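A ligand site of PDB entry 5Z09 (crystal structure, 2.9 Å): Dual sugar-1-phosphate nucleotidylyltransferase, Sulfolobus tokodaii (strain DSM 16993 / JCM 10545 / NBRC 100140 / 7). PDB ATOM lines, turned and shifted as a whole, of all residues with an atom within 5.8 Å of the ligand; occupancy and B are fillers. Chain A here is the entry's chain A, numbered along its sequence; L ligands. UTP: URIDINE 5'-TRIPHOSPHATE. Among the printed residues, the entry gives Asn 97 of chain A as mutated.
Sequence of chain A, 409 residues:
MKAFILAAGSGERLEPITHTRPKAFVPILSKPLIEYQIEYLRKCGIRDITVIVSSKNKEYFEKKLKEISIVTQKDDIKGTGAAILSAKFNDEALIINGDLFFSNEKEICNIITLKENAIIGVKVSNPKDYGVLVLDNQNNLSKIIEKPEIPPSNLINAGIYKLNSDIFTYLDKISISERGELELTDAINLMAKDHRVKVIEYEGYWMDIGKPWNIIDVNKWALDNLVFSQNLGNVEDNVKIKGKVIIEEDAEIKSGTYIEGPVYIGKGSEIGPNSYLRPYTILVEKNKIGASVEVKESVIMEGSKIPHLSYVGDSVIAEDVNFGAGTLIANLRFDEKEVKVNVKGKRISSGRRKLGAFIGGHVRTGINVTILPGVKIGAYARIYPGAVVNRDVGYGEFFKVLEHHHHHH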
ATOM      1  N   LEU A   6      25.848 -23.162   1.567  1.00  0.00           N
ATOM      2  CA  LEU A   6      25.770 -21.698   1.468  1.00  0.00           C
ATOM      3  C   LEU A   6      25.586 -21.207   0.023  1.00  0.00           C
ATOM      4  O   LEU A   6      26.518 -21.252  -0.786  1.00  0.00           O
ATOM      5  CB  LEU A   6      27.033 -21.075   2.053  1.00  0.00           C
ATOM      6  CG  LEU A   6      27.427 -21.593   3.439  1.00  0.00           C
ATOM      7  CD1 LEU A   6      28.797 -21.058   3.820  1.00  0.00           C
ATOM      8  CD2 LEU A   6      26.388 -21.202   4.486  1.00  0.00           C
ATOM      9  N   ALA A   7      24.407 -20.656  -0.248  1.00  0.00           N
ATOM     10  CA  ALA A   7      23.988 -20.343  -1.620  1.00  0.00           C
ATOM     11  C   ALA A   7      23.250 -19.007  -1.732  1.00  0.00           C
ATOM     12  O   ALA A   7      22.307 -18.886  -2.504  1.00  0.00           O
ATOM     13  CB  ALA A   7      23.116 -21.463  -2.114  1.00  0.00           C
ATOM     14  N   ALA A   8      23.708 -18.001  -1.008  1.00  0.00           N
ATOM     15  CA  ALA A   8      23.010 -16.719  -0.935  1.00  0.00           C
ATOM     16  C   ALA A   8      23.898 -15.533  -1.363  1.00  0.00           C
ATOM     17  O   ALA A   8      23.594 -14.372  -1.064  1.00  0.00           O
ATOM     18  CB  ALA A   8      22.512 -16.529   0.491  1.00  0.00           C
ATOM     19  N   GLY A   9      24.976 -15.837  -2.079  1.00  0.00           N
ATOM     20  CA  GLY A   9      25.612 -14.859  -2.947  1.00  0.00           C
ATOM     21  C   GLY A   9      24.718 -14.471  -4.108  1.00  0.00           C
ATOM     22  O   GLY A   9      23.807 -15.220  -4.490  1.00  0.00           O
ATOM     23  N   SER A  10      24.898 -13.250  -4.615  1.00  0.00           N
ATOM     24  CA  SER A  10      24.583 -12.933  -6.003  1.00  0.00           C
ATOM     25  C   SER A  10      25.879 -13.092  -6.747  1.00  0.00           C
ATOM     26  O   SER A  10      26.774 -12.277  -6.589  1.00  0.00           O
ATOM     27  CB  SER A  10      24.073 -11.487  -6.140  1.00  0.00           C
ATOM     28  OG  SER A  10      24.685 -10.651  -5.185  1.00  0.00           O
ATOM     29  N   GLY A  11      26.053 -14.252  -7.375  1.00  0.00           N
ATOM     30  CA  GLY A  11      27.217 -14.505  -8.211  1.00  0.00           C
ATOM     31  C   GLY A  11      27.324 -13.475  -9.301  1.00  0.00           C
ATOM     32  O   GLY A  11      26.929 -13.717 -10.442  1.00  0.00           O
ATOM     33  N   GLU A  12      27.912 -12.324  -8.944  1.00  0.00           N
ATOM     34  CA  GLU A  12      28.122 -11.235  -9.878  1.00  0.00           C
ATOM     35  C   GLU A  12      29.182 -11.624 -10.913  1.00  0.00           C
ATOM     36  O   GLU A  12      29.005 -11.381 -12.106  1.00  0.00           O
ATOM     37  CB  GLU A  12      28.578  -9.979  -9.131  1.00  0.00           C
ATOM     38  CG  GLU A  12      28.042  -8.679  -9.710  1.00  0.00           C
ATOM     39  CD  GLU A  12      28.665  -7.455  -9.054  1.00  0.00           C
ATOM     40  OE1 GLU A  12      29.341  -6.674  -9.772  1.00  0.00           O
ATOM     41  OE2 GLU A  12      28.529  -7.334  -7.810  1.00  0.00           O
ATOM     42  N   ARG A  13      30.220 -12.316 -10.458  1.00  0.00           N
ATOM     43  CA  ARG A  13      31.308 -12.727 -11.354  1.00  0.00           C
ATOM     44  C   ARG A  13      30.866 -13.730 -12.412  1.00  0.00           C
ATOM     45  O   ARG A  13      31.526 -13.878 -13.450  1.00  0.00           O
ATOM     46  CB  ARG A  13      32.453 -13.311 -10.552  1.00  0.00           C
ATOM     47  CG  ARG A  13      33.188 -12.288  -9.714  1.00  0.00           C
ATOM     48  CD  ARG A  13      34.336 -12.902  -8.927  1.00  0.00           C
ATOM     49  NE  ARG A  13      33.864 -13.892  -7.954  1.00  0.00           N
ATOM     50  CZ  ARG A  13      34.316 -15.137  -7.846  1.00  0.00           C
ATOM     51  NH1 ARG A  13      35.350 -15.559  -8.594  1.00  0.00           N
ATOM     52  NH2 ARG A  13      33.752 -15.966  -6.981  1.00  0.00           N
ATOM     53  N   LEU A  14      29.696 -14.356 -12.192  1.00  0.00           N
ATOM     54  CA  LEU A  14      29.144 -15.351 -13.121  1.00  0.00           C
ATOM     55  C   LEU A  14      28.041 -14.795 -14.008  1.00  0.00           C
ATOM     56  O   LEU A  14      27.319 -15.558 -14.669  1.00  0.00           O
ATOM     57  CB  LEU A  14      28.586 -16.526 -12.335  1.00  0.00           C
ATOM     58  CG  LEU A  14      28.621 -17.884 -13.052  1.00  0.00           C
ATOM     59  CD1 LEU A  14      30.042 -18.405 -13.093  1.00  0.00           C
ATOM     60  CD2 LEU A  14      27.693 -18.855 -12.345  1.00  0.00           C
ATOM     61  N   LYS A  23      23.385 -19.360  -8.730  1.00  0.00           N
ATOM     62  CA  LYS A  23      24.546 -20.120  -9.205  1.00  0.00           C
ATOM     63  C   LYS A  23      24.367 -21.592  -8.832  1.00  0.00           C
ATOM     64  O   LYS A  23      24.908 -22.478  -9.513  1.00  0.00           O
ATOM     65  CB  LYS A  23      25.840 -19.538  -8.616  1.00  0.00           C
ATOM     66  CG  LYS A  23      26.990 -20.510  -8.601  1.00  0.00           C
ATOM     67  CD  LYS A  23      28.330 -19.803  -8.719  1.00  0.00           C
ATOM     68  CE  LYS A  23      28.493 -18.639  -7.765  1.00  0.00           C
ATOM     69  NZ  LYS A  23      29.903 -18.169  -7.790  1.00  0.00           N
ATOM     70  N   ILE A  52      21.196 -22.398   2.656  1.00  0.00           N
ATOM     71  CA  ILE A  52      21.038 -20.978   2.984  1.00  0.00           C
ATOM     72  C   ILE A  52      20.984 -20.181   1.686  1.00  0.00           C
ATOM     73  O   ILE A  52      21.966 -20.126   0.947  1.00  0.00           O
ATOM     74  CB  ILE A  52      22.192 -20.425   3.837  1.00  0.00           C
ATOM     75  CG1 ILE A  52      22.476 -21.325   5.054  1.00  0.00           C
ATOM     76  CG2 ILE A  52      21.881 -19.005   4.291  1.00  0.00           C
ATOM     77  CD1 ILE A  52      21.274 -21.546   5.950  1.00  0.00           C
ATOM     78  N   GLN A  73      18.679 -15.797   4.343  1.00  0.00           N
ATOM     79  CA  GLN A  73      19.741 -15.120   5.063  1.00  0.00           C
ATOM     80  C   GLN A  73      19.193 -13.808   5.612  1.00  0.00           C
ATOM     81  O   GLN A  73      18.181 -13.316   5.114  1.00  0.00           O
ATOM     82  CB  GLN A  73      20.908 -14.839   4.125  1.00  0.00           C
ATOM     83  CG  GLN A  73      22.241 -14.676   4.816  1.00  0.00           C
ATOM     84  CD  GLN A  73      23.339 -14.307   3.850  1.00  0.00           C
ATOM     85  OE1 GLN A  73      23.803 -15.131   3.066  1.00  0.00           O
ATOM     86  NE2 GLN A  73      23.804 -13.059   3.916  1.00  0.00           N
ATOM     87  N   ILE A  77      23.237  -7.594   6.683  1.00  0.00           N
ATOM     88  CA  ILE A  77      24.650  -7.724   6.354  1.00  0.00           C
ATOM     89  C   ILE A  77      24.904  -8.961   5.502  1.00  0.00           C
ATOM     90  O   ILE A  77      24.244  -9.988   5.681  1.00  0.00           O
ATOM     91  CB  ILE A  77      25.530  -7.726   7.621  1.00  0.00           C
ATOM     92  CG1 ILE A  77      27.005  -7.561   7.252  1.00  0.00           C
ATOM     93  CG2 ILE A  77      25.328  -9.005   8.422  1.00  0.00           C
ATOM     94  CD1 ILE A  77      27.381  -6.226   6.629  1.00  0.00           C
ATOM     95  N   LYS A  78      25.791  -8.825   4.520  1.00  0.00           N
ATOM     96  CA  LYS A  78      26.129  -9.903   3.587  1.00  0.00           C
ATOM     97  C   LYS A  78      27.322 -10.711   4.089  1.00  0.00           C
ATOM     98  O   LYS A  78      28.029 -10.273   4.999  1.00  0.00           O
ATOM     99  CB  LYS A  78      26.463  -9.346   2.191  1.00  0.00           C
ATOM    100  CG  LYS A  78      25.363  -8.499   1.557  1.00  0.00           C
ATOM    101  CD  LYS A  78      24.434  -9.319   0.655  1.00  0.00           C
ATOM    102  CE  LYS A  78      23.244  -8.503   0.165  1.00  0.00           C
ATOM    103  NZ  LYS A  78      21.986  -8.875   0.872  1.00  0.00           N
ATOM    104  N   GLY A  79      27.563 -11.857   3.455  1.00  0.00           N
ATOM    105  CA  GLY A  79      28.779 -12.641   3.667  1.00  0.00           C
ATOM    106  C   GLY A  79      28.481 -14.092   3.999  1.00  0.00           C
ATOM    107  O   GLY A  79      27.399 -14.417   4.517  1.00  0.00           O
ATOM    108  N   THR A  80      29.457 -14.968   3.751  1.00  0.00           N
ATOM    109  CA  THR A  80      29.394 -16.360   4.203  1.00  0.00           C
ATOM    110  C   THR A  80      29.200 -16.462   5.721  1.00  0.00           C
ATOM    111  O   THR A  80      28.502 -17.345   6.218  1.00  0.00           O
ATOM    112  CB  THR A  80      30.678 -17.137   3.860  1.00  0.00           C
ATOM    113  OG1 THR A  80      31.827 -16.353   4.205  1.00  0.00           O
ATOM    114  CG2 THR A  80      30.728 -17.476   2.383  1.00  0.00           C
ATOM    115  N   ALA A  82      27.548 -14.185   7.514  1.00  0.00           N
ATOM    116  CA  ALA A  82      26.143 -13.835   7.719  1.00  0.00           C
ATOM    117  C   ALA A  82      25.217 -15.008   7.377  1.00  0.00           C
ATOM    118  O   ALA A  82      24.103 -15.116   7.910  1.00  0.00           O
ATOM    119  CB  ALA A  82      25.769 -12.611   6.900  1.00  0.00           C
ATOM    120  N   ALA A  83      25.687 -15.881   6.504  1.00  0.00           N
ATOM    121  CA  ALA A  83      24.903 -17.021   6.040  1.00  0.00           C
ATOM    122  C   ALA A  83      24.649 -18.056   7.154  1.00  0.00           C
ATOM    123  O   ALA A  83      23.482 -18.378   7.436  1.00  0.00           O
ATOM    124  CB  ALA A  83      25.555 -17.673   4.824  1.00  0.00           C
ATOM    125  N   ASN A  97      30.392 -24.660   0.744  1.00  0.00           N
ATOM    126  CA  ASN A  97      30.117 -23.523  -0.158  1.00  0.00           C
ATOM    127  C   ASN A  97      29.334 -23.955  -1.394  1.00  0.00           C
ATOM    128  O   ASN A  97      29.755 -24.861  -2.123  1.00  0.00           O
ATOM    129  CB  ASN A  97      31.406 -22.867  -0.622  1.00  0.00           C
ATOM    130  CG  ASN A  97      31.983 -21.937   0.398  1.00  0.00           C
ATOM    131  OD1 ASN A  97      31.272 -21.403   1.247  1.00  0.00           O
ATOM    132  ND2 ASN A  97      33.275 -21.693   0.291  1.00  0.00           N
ATOM    133  N   GLY A  98      28.243 -23.239  -1.664  1.00  0.00           N
ATOM    134  CA  GLY A  98      27.277 -23.672  -2.664  1.00  0.00           C
ATOM    135  C   GLY A  98      27.698 -23.395  -4.104  1.00  0.00           C
ATOM    136  O   GLY A  98      26.923 -23.592  -5.017  1.00  0.00           O
ATOM    137  N   ASP A  99      28.970 -23.036  -4.295  1.00  0.00           N
ATOM    138  CA  ASP A  99      29.533 -22.812  -5.608  1.00  0.00           C
ATOM    139  C   ASP A  99      30.642 -23.803  -5.952  1.00  0.00           C
ATOM    140  O   ASP A  99      31.443 -23.569  -6.870  1.00  0.00           O
ATOM    141  CB  ASP A  99      30.030 -21.373  -5.712  1.00  0.00           C
ATOM    142  CG  ASP A  99      31.195 -21.079  -4.780  1.00  0.00           C
ATOM    143  OD1 ASP A  99      31.592 -21.960  -4.024  1.00  0.00           O
ATOM    144  OD2 ASP A  99      31.717 -19.957  -4.805  1.00  0.00           O
ATOM    145  N   ARG A 179      35.453  -5.441   2.092  1.00  0.00           N
ATOM    146  CA  ARG A 179      34.435  -5.425   1.025  1.00  0.00           C
ATOM    147  C   ARG A 179      33.015  -5.440   1.584  1.00  0.00           C
ATOM    148  O   ARG A 179      32.064  -5.648   0.836  1.00  0.00           O
ATOM    149  CB  ARG A 179      34.636  -6.582   0.044  1.00  0.00           C
ATOM    150  CG  ARG A 179      34.849  -7.927   0.675  1.00  0.00           C
ATOM    151  CD  ARG A 179      34.962  -9.029  -0.351  1.00  0.00           C
ATOM    152  NE  ARG A 179      34.641 -10.346   0.206  1.00  0.00           N
ATOM    153  CZ  ARG A 179      34.478 -11.447  -0.515  1.00  0.00           C
ATOM    154  NH1 ARG A 179      34.674 -11.424  -1.834  1.00  0.00           N
ATOM    155  NH2 ARG A 179      34.127 -12.580   0.062  1.00  0.00           N
ATOM    156  N   GLU A 181      31.561  -7.158   4.105  1.00  0.00           N
ATOM    157  CA  GLU A 181      30.990  -8.498   4.304  1.00  0.00           C
ATOM    158  C   GLU A 181      31.461  -9.142   5.621  1.00  0.00           C
ATOM    159  O   GLU A 181      32.459  -8.727   6.202  1.00  0.00           O
ATOM    160  CB  GLU A 181      31.335  -9.395   3.118  1.00  0.00           C
ATOM    161  CG  GLU A 181      30.462  -9.151   1.902  1.00  0.00           C
ATOM    162  CD  GLU A 181      30.719 -10.140   0.778  1.00  0.00           C
ATOM    163  OE1 GLU A 181      31.896 -10.409   0.478  1.00  0.00           O
ATOM    164  OE2 GLU A 181      29.731 -10.669   0.229  1.00  0.00           O
ATOM    165  N   GLU A 183      32.929 -12.187   6.757  1.00  0.00           N
ATOM    166  CA  GLU A 183      33.645 -13.347   6.269  1.00  0.00           C
ATOM    167  C   GLU A 183      33.670 -14.460   7.319  1.00  0.00           C
ATOM    168  O   GLU A 183      34.298 -14.308   8.360  1.00  0.00           O
ATOM    169  CB  GLU A 183      35.072 -12.909   5.925  1.00  0.00           C
ATOM    170  CG  GLU A 183      35.412 -12.995   4.460  1.00  0.00           C
ATOM    171  CD  GLU A 183      34.477 -12.176   3.604  1.00  0.00           C
ATOM    172  OE1 GLU A 183      33.487 -12.754   3.096  1.00  0.00           O
ATOM    173  OE2 GLU A 183      34.734 -10.954   3.444  1.00  0.00           O
ATOM    174  N   GLY A 210      33.217 -19.743 -10.300  1.00  0.00           N
ATOM    175  CA  GLY A 210      33.261 -18.304 -10.044  1.00  0.00           C
ATOM    176  C   GLY A 210      33.021 -17.505 -11.296  1.00  0.00           C
ATOM    177  O   GLY A 210      32.218 -16.592 -11.290  1.00  0.00           O
ATOM    178  N   LYS A 344      33.088  -8.152 -12.972  1.00  0.00           N
ATOM    179  CA  LYS A 344      32.878  -7.061 -12.022  1.00  0.00           C
ATOM    180  C   LYS A 344      33.656  -5.822 -12.455  1.00  0.00           C
ATOM    181  O   LYS A 344      34.386  -5.222 -11.659  1.00  0.00           O
ATOM    182  CB  LYS A 344      33.309  -7.448 -10.602  1.00  0.00           C
ATOM    183  CG  LYS A 344      32.472  -8.539  -9.963  1.00  0.00           C
ATOM    184  CD  LYS A 344      32.866  -8.761  -8.526  1.00  0.00           C
ATOM    185  CE  LYS A 344      32.007  -7.984  -7.560  1.00  0.00           C
ATOM    186  NZ  LYS A 344      32.446  -8.193  -6.150  1.00  0.00           N
HETATM  187  PA  UTP L   1      31.606 -15.958  -2.465  1.00  0.00           P
HETATM  188  O1A UTP L   1      32.528 -15.389  -1.393  1.00  0.00           O
HETATM  189  O2A UTP L   1      32.145 -16.600  -3.733  1.00  0.00           O
HETATM  190  O3A UTP L   1      30.489 -14.876  -2.968  1.00  0.00           O
HETATM  191  O5' UTP L   1      30.798 -17.031  -1.558  1.00  0.00           O
HETATM  192  PB  UTP L   1      29.746 -14.899  -4.428  1.00  0.00           P
HETATM  193  O1B UTP L   1      28.521 -14.009  -4.399  1.00  0.00           O
HETATM  194  O2B UTP L   1      29.519 -16.355  -4.774  1.00  0.00           O
HETATM  195  O3B UTP L   1      30.905 -14.237  -5.362  1.00  0.00           O
HETATM  196  PG  UTP L   1      30.759 -13.074  -6.499  1.00  0.00           P
HETATM  197  O1G UTP L   1      30.693 -13.835  -7.798  1.00  0.00           O
HETATM  198  O2G UTP L   1      32.012 -12.243  -6.346  1.00  0.00           O
HETATM  199  O3G UTP L   1      29.481 -12.311  -6.209  1.00  0.00           O
HETATM  200  C5' UTP L   1      31.057 -18.435  -1.605  1.00  0.00           C
HETATM  201  C4' UTP L   1      29.754 -19.135  -1.291  1.00  0.00           C
HETATM  202  O4' UTP L   1      29.215 -18.446  -0.167  1.00  0.00           O
HETATM  203  C1' UTP L   1      27.877 -18.016  -0.454  1.00  0.00           C
HETATM  204  C2' UTP L   1      27.784 -17.943  -1.946  1.00  0.00           C
HETATM  205  O2' UTP L   1      26.419 -18.162  -2.273  1.00  0.00           O
HETATM  206  C3' UTP L   1      28.756 -19.005  -2.439  1.00  0.00           C
HETATM  207  O3' UTP L   1      28.103 -20.244  -2.733  1.00  0.00           O
HETATM  208  N1  UTP L   1      27.456 -16.731   0.106  1.00  0.00           N
HETATM  209  C6  UTP L   1      28.163 -15.610  -0.086  1.00  0.00           C
HETATM  210  C2  UTP L   1      26.260 -16.663   0.849  1.00  0.00           C
HETATM  211  O2  UTP L   1      25.599 -17.698   1.077  1.00  0.00           O
HETATM  212  N3  UTP L   1      25.835 -15.500   1.326  1.00  0.00           N
HETATM  213  C4  UTP L   1      26.531 -14.381   1.164  1.00  0.00           C
HETATM  214  O4  UTP L   1      26.100 -13.314   1.656  1.00  0.00           O
HETATM  215  C5  UTP L   1      27.730 -14.404   0.460  1.00  0.00           C
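The backbone NH of Gly 98 is in hydrogen-bond range of the backbone carbonyl oxygen of Leu 6 (2.8 Å). The backbone NH (N) of Ala 8 sits at hydrogen-bond distance from the backbone carbonyl oxygen (O) of Ile 52 (3.4 Å). The side-chain amino group (NZ) of Lys 23 is in salt-bridge range of the side-chain carboxylate (OD2) of Asp 99 (3.9 Å). The backbone carbonyl oxygen of Ile 52 is in hydrogen-bond range of the backbone NH of Ala 7 (2.8 Å). The guanidinium group of Arg 179 is in salt-bridge range of the side-chain carboxylate of Glu 181, at 2.8 Å. NH2 of Arg 179 is in salt-bridge range of OE1 of Glu 183, at 3.1 Å.
A nitrogen (N3) of the ligand is in hydrogen-bond range of the side-chain amide oxygen of Gln 73, at 2.7 Å. The backbone carbonyl oxygen (O) of Leu 6 sits at hydrogen-bond distance from an oxygen (O3') of the ligand, at 2.7 Å. O of Ser 10 sits close to O3G of the ligand (2.7 Å). An oxygen (O4) of the ligand is in hydrogen-bond range of the backbone NH (N) of Gly 79, at 2.7 Å. An oxygen (O2') of the ligand is in hydrogen-bond range of the backbone NH (N) of Gly 9 (2.7 Å). N of Ala 8 lies within hydrogen-bond range of O2 of the ligand (2.8 Å). A nitrogen (N3) of the ligand lies close to the backbone carbonyl oxygen (O) of Ala 8 (3.5 Å). N of Arg 13 is in hydrogen-bond range of O1G of the ligand (3.1 Å). NE of Arg 13 is in salt-bridge range of O2G of the ligand, at 3.0 Å. An oxygen (O3G) of the ligand is in hydrogen-bond range of the backbone NH of Glu 12 (3.2 Å). An oxygen (O3') of the ligand lies within hydrogen-bond range of the backbone NH of Gly 98, 3.2 Å away. The backbone NH (N) of Asp 99 sits at hydrogen-bond distance from an oxygen (O3') of the ligand (3.3 Å). O2 of the ligand sits at hydrogen-bond distance from N of Ala 7, 3.5 Å away. O2B of the ligand is in salt-bridge range of NZ of Lys 23 (3.5 Å). An oxygen (O1A) of the ligand lies within salt-bridge range of the guanidinium group of Arg 179, at 3.5 Å.
Merely in contact with the ligand: Gly 11, Lys 78, Thr 80, Ala 83 and Asn 97. Of the 26 residues printed, 18 come within 4 Å of the ligand. The nearest printed residue that does not touch the ligand is Lys 344 (4.1 Å).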
